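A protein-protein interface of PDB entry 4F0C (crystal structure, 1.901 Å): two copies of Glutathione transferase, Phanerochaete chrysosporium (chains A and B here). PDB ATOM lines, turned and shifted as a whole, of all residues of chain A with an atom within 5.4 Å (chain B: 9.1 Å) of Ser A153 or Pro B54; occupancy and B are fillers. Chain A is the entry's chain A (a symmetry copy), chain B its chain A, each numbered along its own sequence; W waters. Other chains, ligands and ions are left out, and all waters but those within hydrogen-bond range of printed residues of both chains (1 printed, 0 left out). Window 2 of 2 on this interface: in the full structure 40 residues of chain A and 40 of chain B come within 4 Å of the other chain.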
ATOM      1  N   TRP A 105     -24.653 -23.352   2.737  1.00  0.00           N
ATOM      2  CA  TRP A 105     -25.508 -22.419   2.019  1.00  0.00           C
ATOM      3  C   TRP A 105     -26.780 -22.095   2.803  1.00  0.00           C
ATOM      4  O   TRP A 105     -27.248 -20.961   2.762  1.00  0.00           O
ATOM      5  CB  TRP A 105     -25.821 -22.929   0.606  1.00  0.00           C
ATOM      6  CG  TRP A 105     -24.619 -22.684  -0.302  1.00  0.00           C
ATOM      7  CD1 TRP A 105     -23.674 -23.595  -0.674  1.00  0.00           C
ATOM      8  CD2 TRP A 105     -24.234 -21.431  -0.871  1.00  0.00           C
ATOM      9  NE1 TRP A 105     -22.723 -22.988  -1.477  1.00  0.00           N
ATOM     10  CE2 TRP A 105     -23.047 -21.654  -1.605  1.00  0.00           C
ATOM     11  CE3 TRP A 105     -24.803 -20.141  -0.853  1.00  0.00           C
ATOM     12  CZ2 TRP A 105     -22.399 -20.631  -2.324  1.00  0.00           C
ATOM     13  CZ3 TRP A 105     -24.147 -19.102  -1.561  1.00  0.00           C
ATOM     14  CH2 TRP A 105     -22.949 -19.361  -2.265  1.00  0.00           C
ATOM     15  N   PHE A 148     -27.069 -10.205  -3.377  1.00  0.00           N
ATOM     16  CA  PHE A 148     -27.316 -10.485  -4.799  1.00  0.00           C
ATOM     17  C   PHE A 148     -25.993 -10.641  -5.574  1.00  0.00           C
ATOM     18  O   PHE A 148     -25.860 -11.542  -6.404  1.00  0.00           O
ATOM     19  CB  PHE A 148     -28.120  -9.359  -5.453  1.00  0.00           C
ATOM     20  CG  PHE A 148     -29.599  -9.392  -5.148  1.00  0.00           C
ATOM     21  CD1 PHE A 148     -30.178 -10.468  -4.483  1.00  0.00           C
ATOM     22  CD2 PHE A 148     -30.417  -8.324  -5.537  1.00  0.00           C
ATOM     23  CE1 PHE A 148     -31.544 -10.470  -4.209  1.00  0.00           C
ATOM     24  CE2 PHE A 148     -31.781  -8.327  -5.262  1.00  0.00           C
ATOM     25  CZ  PHE A 148     -32.343  -9.397  -4.608  1.00  0.00           C
ATOM     26  N   GLY A 149     -25.035  -9.755  -5.311  1.00  0.00           N
ATOM     27  CA  GLY A 149     -23.704  -9.827  -5.940  1.00  0.00           C
ATOM     28  C   GLY A 149     -22.989 -11.146  -5.628  1.00  0.00           C
ATOM     29  O   GLY A 149     -22.387 -11.788  -6.506  1.00  0.00           O
ATOM     30  N   VAL A 150     -23.057 -11.559  -4.377  1.00  0.00           N
ATOM     31  CA  VAL A 150     -22.460 -12.830  -3.956  1.00  0.00           C
ATOM     32  C   VAL A 150     -23.103 -14.002  -4.720  1.00  0.00           C
ATOM     33  O   VAL A 150     -22.401 -14.869  -5.296  1.00  0.00           O
ATOM     34  CB  VAL A 150     -22.584 -13.027  -2.418  1.00  0.00           C
ATOM     35  CG1 VAL A 150     -22.188 -14.492  -2.012  1.00  0.00           C
ATOM     36  CG2 VAL A 150     -21.723 -11.985  -1.658  1.00  0.00           C
ATOM     37  N   LEU A 151     -24.431 -14.031  -4.737  1.00  0.00           N
ATOM     38  CA  LEU A 151     -25.163 -15.094  -5.449  1.00  0.00           C
ATOM     39  C   LEU A 151     -24.830 -15.051  -6.944  1.00  0.00           C
ATOM     40  O   LEU A 151     -24.629 -16.083  -7.576  1.00  0.00           O
ATOM     41  CB  LEU A 151     -26.679 -14.967  -5.219  1.00  0.00           C
ATOM     42  CG  LEU A 151     -27.123 -15.296  -3.784  1.00  0.00           C
ATOM     43  CD1 LEU A 151     -28.585 -14.855  -3.574  1.00  0.00           C
ATOM     44  CD2 LEU A 151     -26.942 -16.794  -3.495  1.00  0.00           C
ATOM     45  N   GLU A 152     -24.716 -13.845  -7.491  1.00  0.00           N
ATOM     46  CA  GLU A 152     -24.348 -13.677  -8.901  1.00  0.00           C
ATOM     47  C   GLU A 152     -22.980 -14.282  -9.213  1.00  0.00           C
ATOM     48  O   GLU A 152     -22.805 -14.949 -10.242  1.00  0.00           O
ATOM     49  CB  GLU A 152     -24.343 -12.192  -9.268  1.00  0.00           C
ATOM     50  CG  GLU A 152     -24.053 -11.903 -10.760  1.00  0.00           C
ATOM     51  CD  GLU A 152     -25.166 -12.334 -11.688  1.00  0.00           C
ATOM     52  OE1 GLU A 152     -26.328 -12.422 -11.251  1.00  0.00           O
ATOM     53  OE2 GLU A 152     -24.883 -12.588 -12.873  1.00  0.00           O
ATOM     54  N   SER A 153     -22.023 -14.050  -8.314  1.00  0.00           N
ATOM     55  CA  SER A 153     -20.649 -14.509  -8.498  1.00  0.00           C
ATOM     56  C   SER A 153     -20.559 -16.029  -8.585  1.00  0.00           C
ATOM     57  O   SER A 153     -19.665 -16.545  -9.253  1.00  0.00           O
ATOM     58  CB  SER A 153     -19.709 -13.984  -7.393  1.00  0.00           C
ATOM     59  OG  SER A 153     -19.918 -14.662  -6.144  1.00  0.00           O
ATOM     60  N   VAL A 154     -21.475 -16.745  -7.938  1.00  0.00           N
ATOM     61  CA  VAL A 154     -21.453 -18.211  -8.061  1.00  0.00           C
ATOM     62  C   VAL A 154     -22.420 -18.757  -9.115  1.00  0.00           C
ATOM     63  O   VAL A 154     -22.063 -19.693  -9.832  1.00  0.00           O
ATOM     64  CB  VAL A 154     -21.639 -18.978  -6.688  1.00  0.00           C
ATOM     65  CG1 VAL A 154     -20.723 -18.413  -5.621  1.00  0.00           C
ATOM     66  CG2 VAL A 154     -23.071 -18.949  -6.212  1.00  0.00           C
ATOM     67  N   LEU A 155     -23.619 -18.176  -9.220  1.00  0.00           N
ATOM     68  CA  LEU A 155     -24.634 -18.689 -10.160  1.00  0.00           C
ATOM     69  C   LEU A 155     -24.287 -18.421 -11.622  1.00  0.00           C
ATOM     70  O   LEU A 155     -24.912 -18.977 -12.534  1.00  0.00           O
ATOM     71  CB  LEU A 155     -26.019 -18.126  -9.813  1.00  0.00           C
ATOM     72  CG  LEU A 155     -26.515 -18.667  -8.452  1.00  0.00           C
ATOM     73  CD1 LEU A 155     -27.705 -17.857  -7.986  1.00  0.00           C
ATOM     74  CD2 LEU A 155     -26.880 -20.145  -8.586  1.00  0.00           C
ATOM     75  N   SER A 156     -23.306 -17.560 -11.876  1.00  0.00           N
ATOM     76  CA  SER A 156     -22.886 -17.392 -13.273  1.00  0.00           C
ATOM     77  C   SER A 156     -22.073 -18.603 -13.717  1.00  0.00           C
ATOM     78  O   SER A 156     -21.773 -18.744 -14.886  1.00  0.00           O
ATOM     79  CB  SER A 156     -22.043 -16.117 -13.448  1.00  0.00           C
ATOM     80  OG  SER A 156     -20.923 -16.168 -12.570  1.00  0.00           O
ATOM     81  N   GLN A 157     -21.696 -19.471 -12.783  1.00  0.00           N
ATOM     82  CA  GLN A 157     -20.844 -20.601 -13.111  1.00  0.00           C
ATOM     83  C   GLN A 157     -21.387 -21.912 -12.564  1.00  0.00           C
ATOM     84  O   GLN A 157     -20.733 -22.930 -12.676  1.00  0.00           O
ATOM     85  CB  GLN A 157     -19.442 -20.369 -12.537  1.00  0.00           C
ATOM     86  CG  GLN A 157     -18.769 -19.163 -13.164  1.00  0.00           C
ATOM     87  CD  GLN A 157     -17.293 -19.134 -12.915  1.00  0.00           C
ATOM     88  OE1 GLN A 157     -16.826 -19.447 -11.819  1.00  0.00           O
ATOM     89  NE2 GLN A 157     -16.536 -18.756 -13.935  1.00  0.00           N
ATOM     90  N   HIS B  44     -10.558  -9.303   2.758  1.00  0.00           N
ATOM     91  CA  HIS B  44     -11.633 -10.296   2.771  1.00  0.00           C
ATOM     92  C   HIS B  44     -12.527 -10.223   1.519  1.00  0.00           C
ATOM     93  O   HIS B  44     -13.284 -11.155   1.243  1.00  0.00           O
ATOM     94  CB  HIS B  44     -12.469 -10.137   4.045  1.00  0.00           C
ATOM     95  CG  HIS B  44     -13.089  -8.780   4.191  1.00  0.00           C
ATOM     96  ND1 HIS B  44     -12.345  -7.615   4.184  1.00  0.00           N
ATOM     97  CD2 HIS B  44     -14.381  -8.400   4.348  1.00  0.00           C
ATOM     98  CE1 HIS B  44     -13.156  -6.577   4.324  1.00  0.00           C
ATOM     99  NE2 HIS B  44     -14.396  -7.026   4.433  1.00  0.00           N
ATOM    100  N   LYS B  45     -12.428  -9.121   0.772  1.00  0.00           N
ATOM    101  CA  LYS B  45     -13.209  -8.933  -0.452  1.00  0.00           C
ATOM    102  C   LYS B  45     -12.336  -9.107  -1.706  1.00  0.00           C
ATOM    103  O   LYS B  45     -12.803  -8.919  -2.829  1.00  0.00           O
ATOM    104  CB  LYS B  45     -13.874  -7.543  -0.474  1.00  0.00           C
ATOM    105  CG  LYS B  45     -14.813  -7.226   0.713  1.00  0.00           C
ATOM    106  CD  LYS B  45     -15.770  -8.384   1.034  1.00  0.00           C
ATOM    107  CE  LYS B  45     -16.958  -7.903   1.893  1.00  0.00           C
ATOM    108  NZ  LYS B  45     -17.879  -9.017   2.290  1.00  0.00           N
ATOM    109  N   SER B  46     -11.067  -9.459  -1.507  1.00  0.00           N
ATOM    110  CA  SER B  46     -10.143  -9.668  -2.625  1.00  0.00           C
ATOM    111  C   SER B  46     -10.290 -11.098  -3.156  1.00  0.00           C
ATOM    112  O   SER B  46     -10.682 -11.991  -2.403  1.00  0.00           O
ATOM    113  CB  SER B  46      -8.699  -9.447  -2.169  1.00  0.00           C
ATOM    114  OG  SER B  46      -8.299 -10.487  -1.286  1.00  0.00           O
ATOM    115  N   PRO B  47      -9.967 -11.316  -4.454  1.00  0.00           N
ATOM    116  CA  PRO B  47      -9.948 -12.654  -5.066  1.00  0.00           C
ATOM    117  C   PRO B  47      -9.226 -13.679  -4.198  1.00  0.00           C
ATOM    118  O   PRO B  47      -9.624 -14.846  -4.152  1.00  0.00           O
ATOM    119  CB  PRO B  47      -9.153 -12.437  -6.363  1.00  0.00           C
ATOM    120  CG  PRO B  47      -9.457 -11.013  -6.740  1.00  0.00           C
ATOM    121  CD  PRO B  47      -9.650 -10.255  -5.437  1.00  0.00           C
ATOM    122  N   PHE B  49      -9.223 -14.057  -1.067  1.00  0.00           N
ATOM    123  CA  PHE B  49     -10.061 -14.642  -0.026  1.00  0.00           C
ATOM    124  C   PHE B  49     -11.434 -15.074  -0.542  1.00  0.00           C
ATOM    125  O   PHE B  49     -11.969 -16.071  -0.074  1.00  0.00           O
ATOM    126  CB  PHE B  49     -10.220 -13.739   1.207  1.00  0.00           C
ATOM    127  CG  PHE B  49     -11.014 -14.374   2.308  1.00  0.00           C
ATOM    128  CD1 PHE B  49     -10.462 -15.379   3.078  1.00  0.00           C
ATOM    129  CD2 PHE B  49     -12.324 -13.991   2.562  1.00  0.00           C
ATOM    130  CE1 PHE B  49     -11.183 -15.987   4.090  1.00  0.00           C
ATOM    131  CE2 PHE B  49     -13.051 -14.588   3.575  1.00  0.00           C
ATOM    132  CZ  PHE B  49     -12.499 -15.600   4.333  1.00  0.00           C
ATOM    133  N   THR B  50     -11.990 -14.363  -1.513  1.00  0.00           N
ATOM    134  CA  THR B  50     -13.301 -14.769  -2.031  1.00  0.00           C
ATOM    135  C   THR B  50     -13.211 -16.120  -2.738  1.00  0.00           C
ATOM    136  O   THR B  50     -14.218 -16.814  -2.911  1.00  0.00           O
ATOM    137  CB  THR B  50     -13.978 -13.688  -2.933  1.00  0.00           C
ATOM    138  OG1 THR B  50     -13.169 -13.428  -4.085  1.00  0.00           O
ATOM    139  CG2 THR B  50     -14.174 -12.397  -2.148  1.00  0.00           C
ATOM    140  N   LYS B  51     -11.996 -16.519  -3.109  1.00  0.00           N
ATOM    141  CA  LYS B  51     -11.798 -17.867  -3.649  1.00  0.00           C
ATOM    142  C   LYS B  51     -12.128 -18.931  -2.599  1.00  0.00           C
ATOM    143  O   LYS B  51     -12.509 -20.060  -2.938  1.00  0.00           O
ATOM    144  CB  LYS B  51     -10.380 -18.046  -4.236  1.00  0.00           C
ATOM    145  CG  LYS B  51      -9.265 -18.294  -3.218  1.00  0.00           C
ATOM    146  CD  LYS B  51      -7.892 -18.327  -3.935  1.00  0.00           C
ATOM    147  CE  LYS B  51      -6.749 -18.594  -2.963  1.00  0.00           C
ATOM    148  NZ  LYS B  51      -5.431 -18.086  -3.436  1.00  0.00           N
ATOM    149  N   TYR B  52     -11.994 -18.564  -1.321  1.00  0.00           N
ATOM    150  CA  TYR B  52     -12.392 -19.436  -0.212  1.00  0.00           C
ATOM    151  C   TYR B  52     -13.833 -19.222   0.222  1.00  0.00           C
ATOM    152  O   TYR B  52     -14.525 -20.172   0.550  1.00  0.00           O
ATOM    153  CB  TYR B  52     -11.498 -19.209   0.997  1.00  0.00           C
ATOM    154  CG  TYR B  52     -10.061 -19.584   0.714  1.00  0.00           C
ATOM    155  CD1 TYR B  52      -9.719 -20.902   0.414  1.00  0.00           C
ATOM    156  CD2 TYR B  52      -9.059 -18.629   0.719  1.00  0.00           C
ATOM    157  CE1 TYR B  52      -8.411 -21.259   0.135  1.00  0.00           C
ATOM    158  CE2 TYR B  52      -7.734 -18.979   0.436  1.00  0.00           C
ATOM    159  CZ  TYR B  52      -7.428 -20.296   0.160  1.00  0.00           C
ATOM    160  OH  TYR B  52      -6.140 -20.665  -0.113  1.00  0.00           O
ATOM    161  N   ASN B  53     -14.269 -17.967   0.260  1.00  0.00           N
ATOM    162  CA  ASN B  53     -15.654 -17.666   0.616  1.00  0.00           C
ATOM    163  C   ASN B  53     -16.211 -16.594  -0.301  1.00  0.00           C
ATOM    164  O   ASN B  53     -15.824 -15.425  -0.200  1.00  0.00           O
ATOM    165  CB  ASN B  53     -15.759 -17.235   2.097  1.00  0.00           C
ATOM    166  CG  ASN B  53     -17.196 -16.920   2.504  1.00  0.00           C
ATOM    167  OD1 ASN B  53     -18.093 -17.045   1.685  1.00  0.00           O
ATOM    168  ND2 ASN B  53     -17.418 -16.543   3.778  1.00  0.00           N
ATOM    169  N   PRO B  54     -17.129 -16.971  -1.217  1.00  0.00           N
ATOM    170  CA  PRO B  54     -17.626 -15.943  -2.144  1.00  0.00           C
ATOM    171  C   PRO B  54     -18.351 -14.823  -1.413  1.00  0.00           C
ATOM    172  O   PRO B  54     -18.431 -13.722  -1.966  1.00  0.00           O
ATOM    173  CB  PRO B  54     -18.601 -16.709  -3.056  1.00  0.00           C
ATOM    174  CG  PRO B  54     -18.968 -17.973  -2.284  1.00  0.00           C
ATOM    175  CD  PRO B  54     -17.749 -18.297  -1.440  1.00  0.00           C
ATOM    176  N   ASN B  55     -18.873 -15.106  -0.218  1.00  0.00           N
ATOM    177  CA  ASN B  55     -19.522 -14.095   0.629  1.00  0.00           C
ATOM    178  C   ASN B  55     -18.498 -13.069   1.172  1.00  0.00           C
ATOM    179  O   ASN B  55     -18.878 -11.968   1.578  1.00  0.00           O
ATOM    180  CB  ASN B  55     -20.311 -14.726   1.782  1.00  0.00           C
ATOM    181  CG  ASN B  55     -21.215 -13.709   2.506  1.00  0.00           C
ATOM    182  OD1 ASN B  55     -21.778 -12.835   1.861  1.00  0.00           O
ATOM    183  ND2 ASN B  55     -21.308 -13.794   3.836  1.00  0.00           N
ATOM    184  N   GLY B  56     -17.206 -13.442   1.184  1.00  0.00           N
ATOM    185  CA  GLY B  56     -16.155 -12.491   1.572  1.00  0.00           C
ATOM    186  C   GLY B  56     -16.255 -12.048   3.040  1.00  0.00           C
ATOM    187  O   GLY B  56     -16.007 -10.882   3.389  1.00  0.00           O
ATOM    188  N   ARG B  57     -16.620 -12.982   3.904  1.00  0.00           N
ATOM    189  CA  ARG B  57     -16.658 -12.732   5.352  1.00  0.00           C
ATOM    190  C   ARG B  57     -15.926 -13.864   6.066  1.00  0.00           C
ATOM    191  O   ARG B  57     -15.853 -14.980   5.561  1.00  0.00           O
ATOM    192  CB  ARG B  57     -18.107 -12.615   5.858  1.00  0.00           C
ATOM    193  CG  ARG B  57     -18.873 -11.444   5.235  1.00  0.00           C
ATOM    194  CD  ARG B  57     -20.279 -11.311   5.889  1.00  0.00           C
ATOM    195  NE  ARG B  57     -20.338 -10.279   6.933  1.00  0.00           N
ATOM    196  CZ  ARG B  57     -21.389 -10.058   7.730  1.00  0.00           C
ATOM    197  NH1 ARG B  57     -22.459 -10.833   7.651  1.00  0.00           N
ATOM    198  NH2 ARG B  57     -21.353  -9.086   8.635  1.00  0.00           N
ATOM    199  N   PRO B  59     -15.497 -16.382   9.523  1.00  0.00           N
ATOM    200  CA  PRO B  59     -14.383 -17.289   9.216  1.00  0.00           C
ATOM    201  C   PRO B  59     -14.560 -18.162   7.960  1.00  0.00           C
ATOM    202  O   PRO B  59     -15.653 -18.293   7.382  1.00  0.00           O
ATOM    203  CB  PRO B  59     -14.359 -18.213  10.428  1.00  0.00           C
ATOM    204  CG  PRO B  59     -15.833 -18.339  10.770  1.00  0.00           C
ATOM    205  CD  PRO B  59     -16.343 -16.911  10.606  1.00  0.00           C
ATOM    206  N   ALA B  60     -13.447 -18.758   7.552  1.00  0.00           N
ATOM    207  CA  ALA B  60     -13.467 -19.868   6.611  1.00  0.00           C
ATOM    208  C   ALA B  60     -12.404 -20.822   7.135  1.00  0.00           C
ATOM    209  O   ALA B  60     -11.465 -20.396   7.825  1.00  0.00           O
ATOM    210  CB  ALA B  60     -13.116 -19.404   5.162  1.00  0.00           C
ATOM    211  N   VAL B  70     -12.774 -26.922   1.932  1.00  0.00           N
ATOM    212  CA  VAL B  70     -13.071 -25.604   2.523  1.00  0.00           C
ATOM    213  C   VAL B  70     -14.521 -25.505   2.965  1.00  0.00           C
ATOM    214  O   VAL B  70     -15.424 -25.882   2.221  1.00  0.00           O
ATOM    215  CB  VAL B  70     -12.841 -24.467   1.475  1.00  0.00           C
ATOM    216  CG1 VAL B  70     -13.303 -23.101   2.037  1.00  0.00           C
ATOM    217  CG2 VAL B  70     -11.361 -24.435   0.996  1.00  0.00           C
ATOM    218  N   VAL B  71     -14.753 -24.960   4.164  1.00  0.00           N
ATOM    219  CA  VAL B  71     -16.098 -24.657   4.628  1.00  0.00           C
ATOM    220  C   VAL B  71     -16.122 -23.237   5.216  1.00  0.00           C
ATOM    221  O   VAL B  71     -15.176 -22.808   5.891  1.00  0.00           O
ATOM    222  CB  VAL B  71     -16.575 -25.681   5.701  1.00  0.00           C
ATOM    223  CG1 VAL B  71     -18.012 -25.356   6.166  1.00  0.00           C
ATOM    224  CG2 VAL B  71     -16.507 -27.127   5.151  1.00  0.00           C
ATOM    225  N   TRP B  72     -17.188 -22.500   4.935  1.00  0.00           N
ATOM    226  CA  TRP B  72     -17.377 -21.189   5.555  1.00  0.00           C
ATOM    227  C   TRP B  72     -18.777 -21.141   6.204  1.00  0.00           C
ATOM    228  O   TRP B  72     -19.499 -22.135   6.142  1.00  0.00           O
ATOM    229  CB  TRP B  72     -17.102 -20.059   4.542  1.00  0.00           C
ATOM    230  CG  TRP B  72     -17.851 -20.198   3.167  1.00  0.00           C
ATOM    231  CD1 TRP B  72     -17.402 -20.852   2.015  1.00  0.00           C
ATOM    232  CD2 TRP B  72     -19.140 -19.640   2.830  1.00  0.00           C
ATOM    233  NE1 TRP B  72     -18.363 -20.727   0.999  1.00  0.00           N
ATOM    234  CE2 TRP B  72     -19.426 -19.998   1.480  1.00  0.00           C
ATOM    235  CE3 TRP B  72     -20.070 -18.853   3.535  1.00  0.00           C
ATOM    236  CZ2 TRP B  72     -20.609 -19.605   0.829  1.00  0.00           C
ATOM    237  CZ3 TRP B  72     -21.254 -18.464   2.885  1.00  0.00           C
ATOM    238  CH2 TRP B  72     -21.511 -18.849   1.539  1.00  0.00           C
ATOM    239  N   GLU B  73     -19.139 -19.999   6.797  1.00  0.00           N
ATOM    240  CA  GLU B  73     -20.204 -19.893   7.808  1.00  0.00           C
ATOM    241  C   GLU B  73     -19.718 -20.566   9.083  1.00  0.00           C
ATOM    242  O   GLU B  73     -19.582 -21.797   9.141  1.00  0.00           O
ATOM    243  CB  GLU B  73     -21.567 -20.461   7.366  1.00  0.00           C
ATOM    244  CG  GLU B  73     -22.330 -19.556   6.376  1.00  0.00           C
ATOM    245  CD  GLU B  73     -22.623 -18.164   6.950  1.00  0.00           C
ATOM    246  OE1 GLU B  73     -23.034 -18.052   8.120  1.00  0.00           O
ATOM    247  OE2 GLU B  73     -22.421 -17.163   6.219  1.00  0.00           O
HETATM  248  O   HOH W   1     -17.942 -13.499  -4.701  1.00  0.00           O
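Among the printed residues, pairs that only touch across the chains: Trp A105 with Trp B72, Val A150 with Pro B54, Val A150 with Asn B55, Ser A153 with Pro B54 and Val A154 with Pro B54.
Of the printed residues of chain B, Trp A105 touches Trp B72.
Ser A153 touches one residue of chain B.
Printed residues of chain B within 4 Å of Val A154: Pro B54.
Of chain A, only Val A150, Ser A153 and Val A154 come within 4 Å of Pro B54.
Of the printed residues of chain A, Asn B55 touches Val A150 (3.6 Å).
Printed residues of chain A within 4 Å of Trp B72: Trp A105 (3.8 Å).
The nearest residue of chain B that does not touch Ser A153 is Asn B55 (6.0 Å).
The nearest residue of chain A that does not touch Pro B54 is Trp A105 (4.2 Å).
The nearest printed residue of chain A that does not touch Trp B72 is Val A150 (5.7 Å).
No position is printed for both chains.
Of the 5 pairs that touch across the chains among the printed residues, none has its exchanged pair printed and touching as well.
Water W1 lies within hydrogen-bond range of OG of Ser A153 (2.7 Å) and O of Pro B54 (2.8 Å).
The backbone carbonyl oxygen (O) of Asn B55 lies within hydrogen-bond range of the side-chain amino group (NZ) of Lys B45.
The backbone carbonyl oxygen of Val A150 is in hydrogen-bond range of the side-chain hydroxyl of Ser A153 (2.6 Å).
The side-chain amide oxygen of Asn B53 lies within hydrogen-bond range of the backbone NH of Asn B55, at 2.8 Å.
Printed residues of chain A that touch a printed residue of chain B: Trp A105, Val A150, Ser A153 and Val A154.
Of the 19 printed residues of chain B, 3 touch a printed residue of chain A.
Printed residues of chain B that touch a printed residue of chain A: Pro B54, Asn B55 and Trp B72.
Among the printed residues, 5 pairs touch across the chains.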
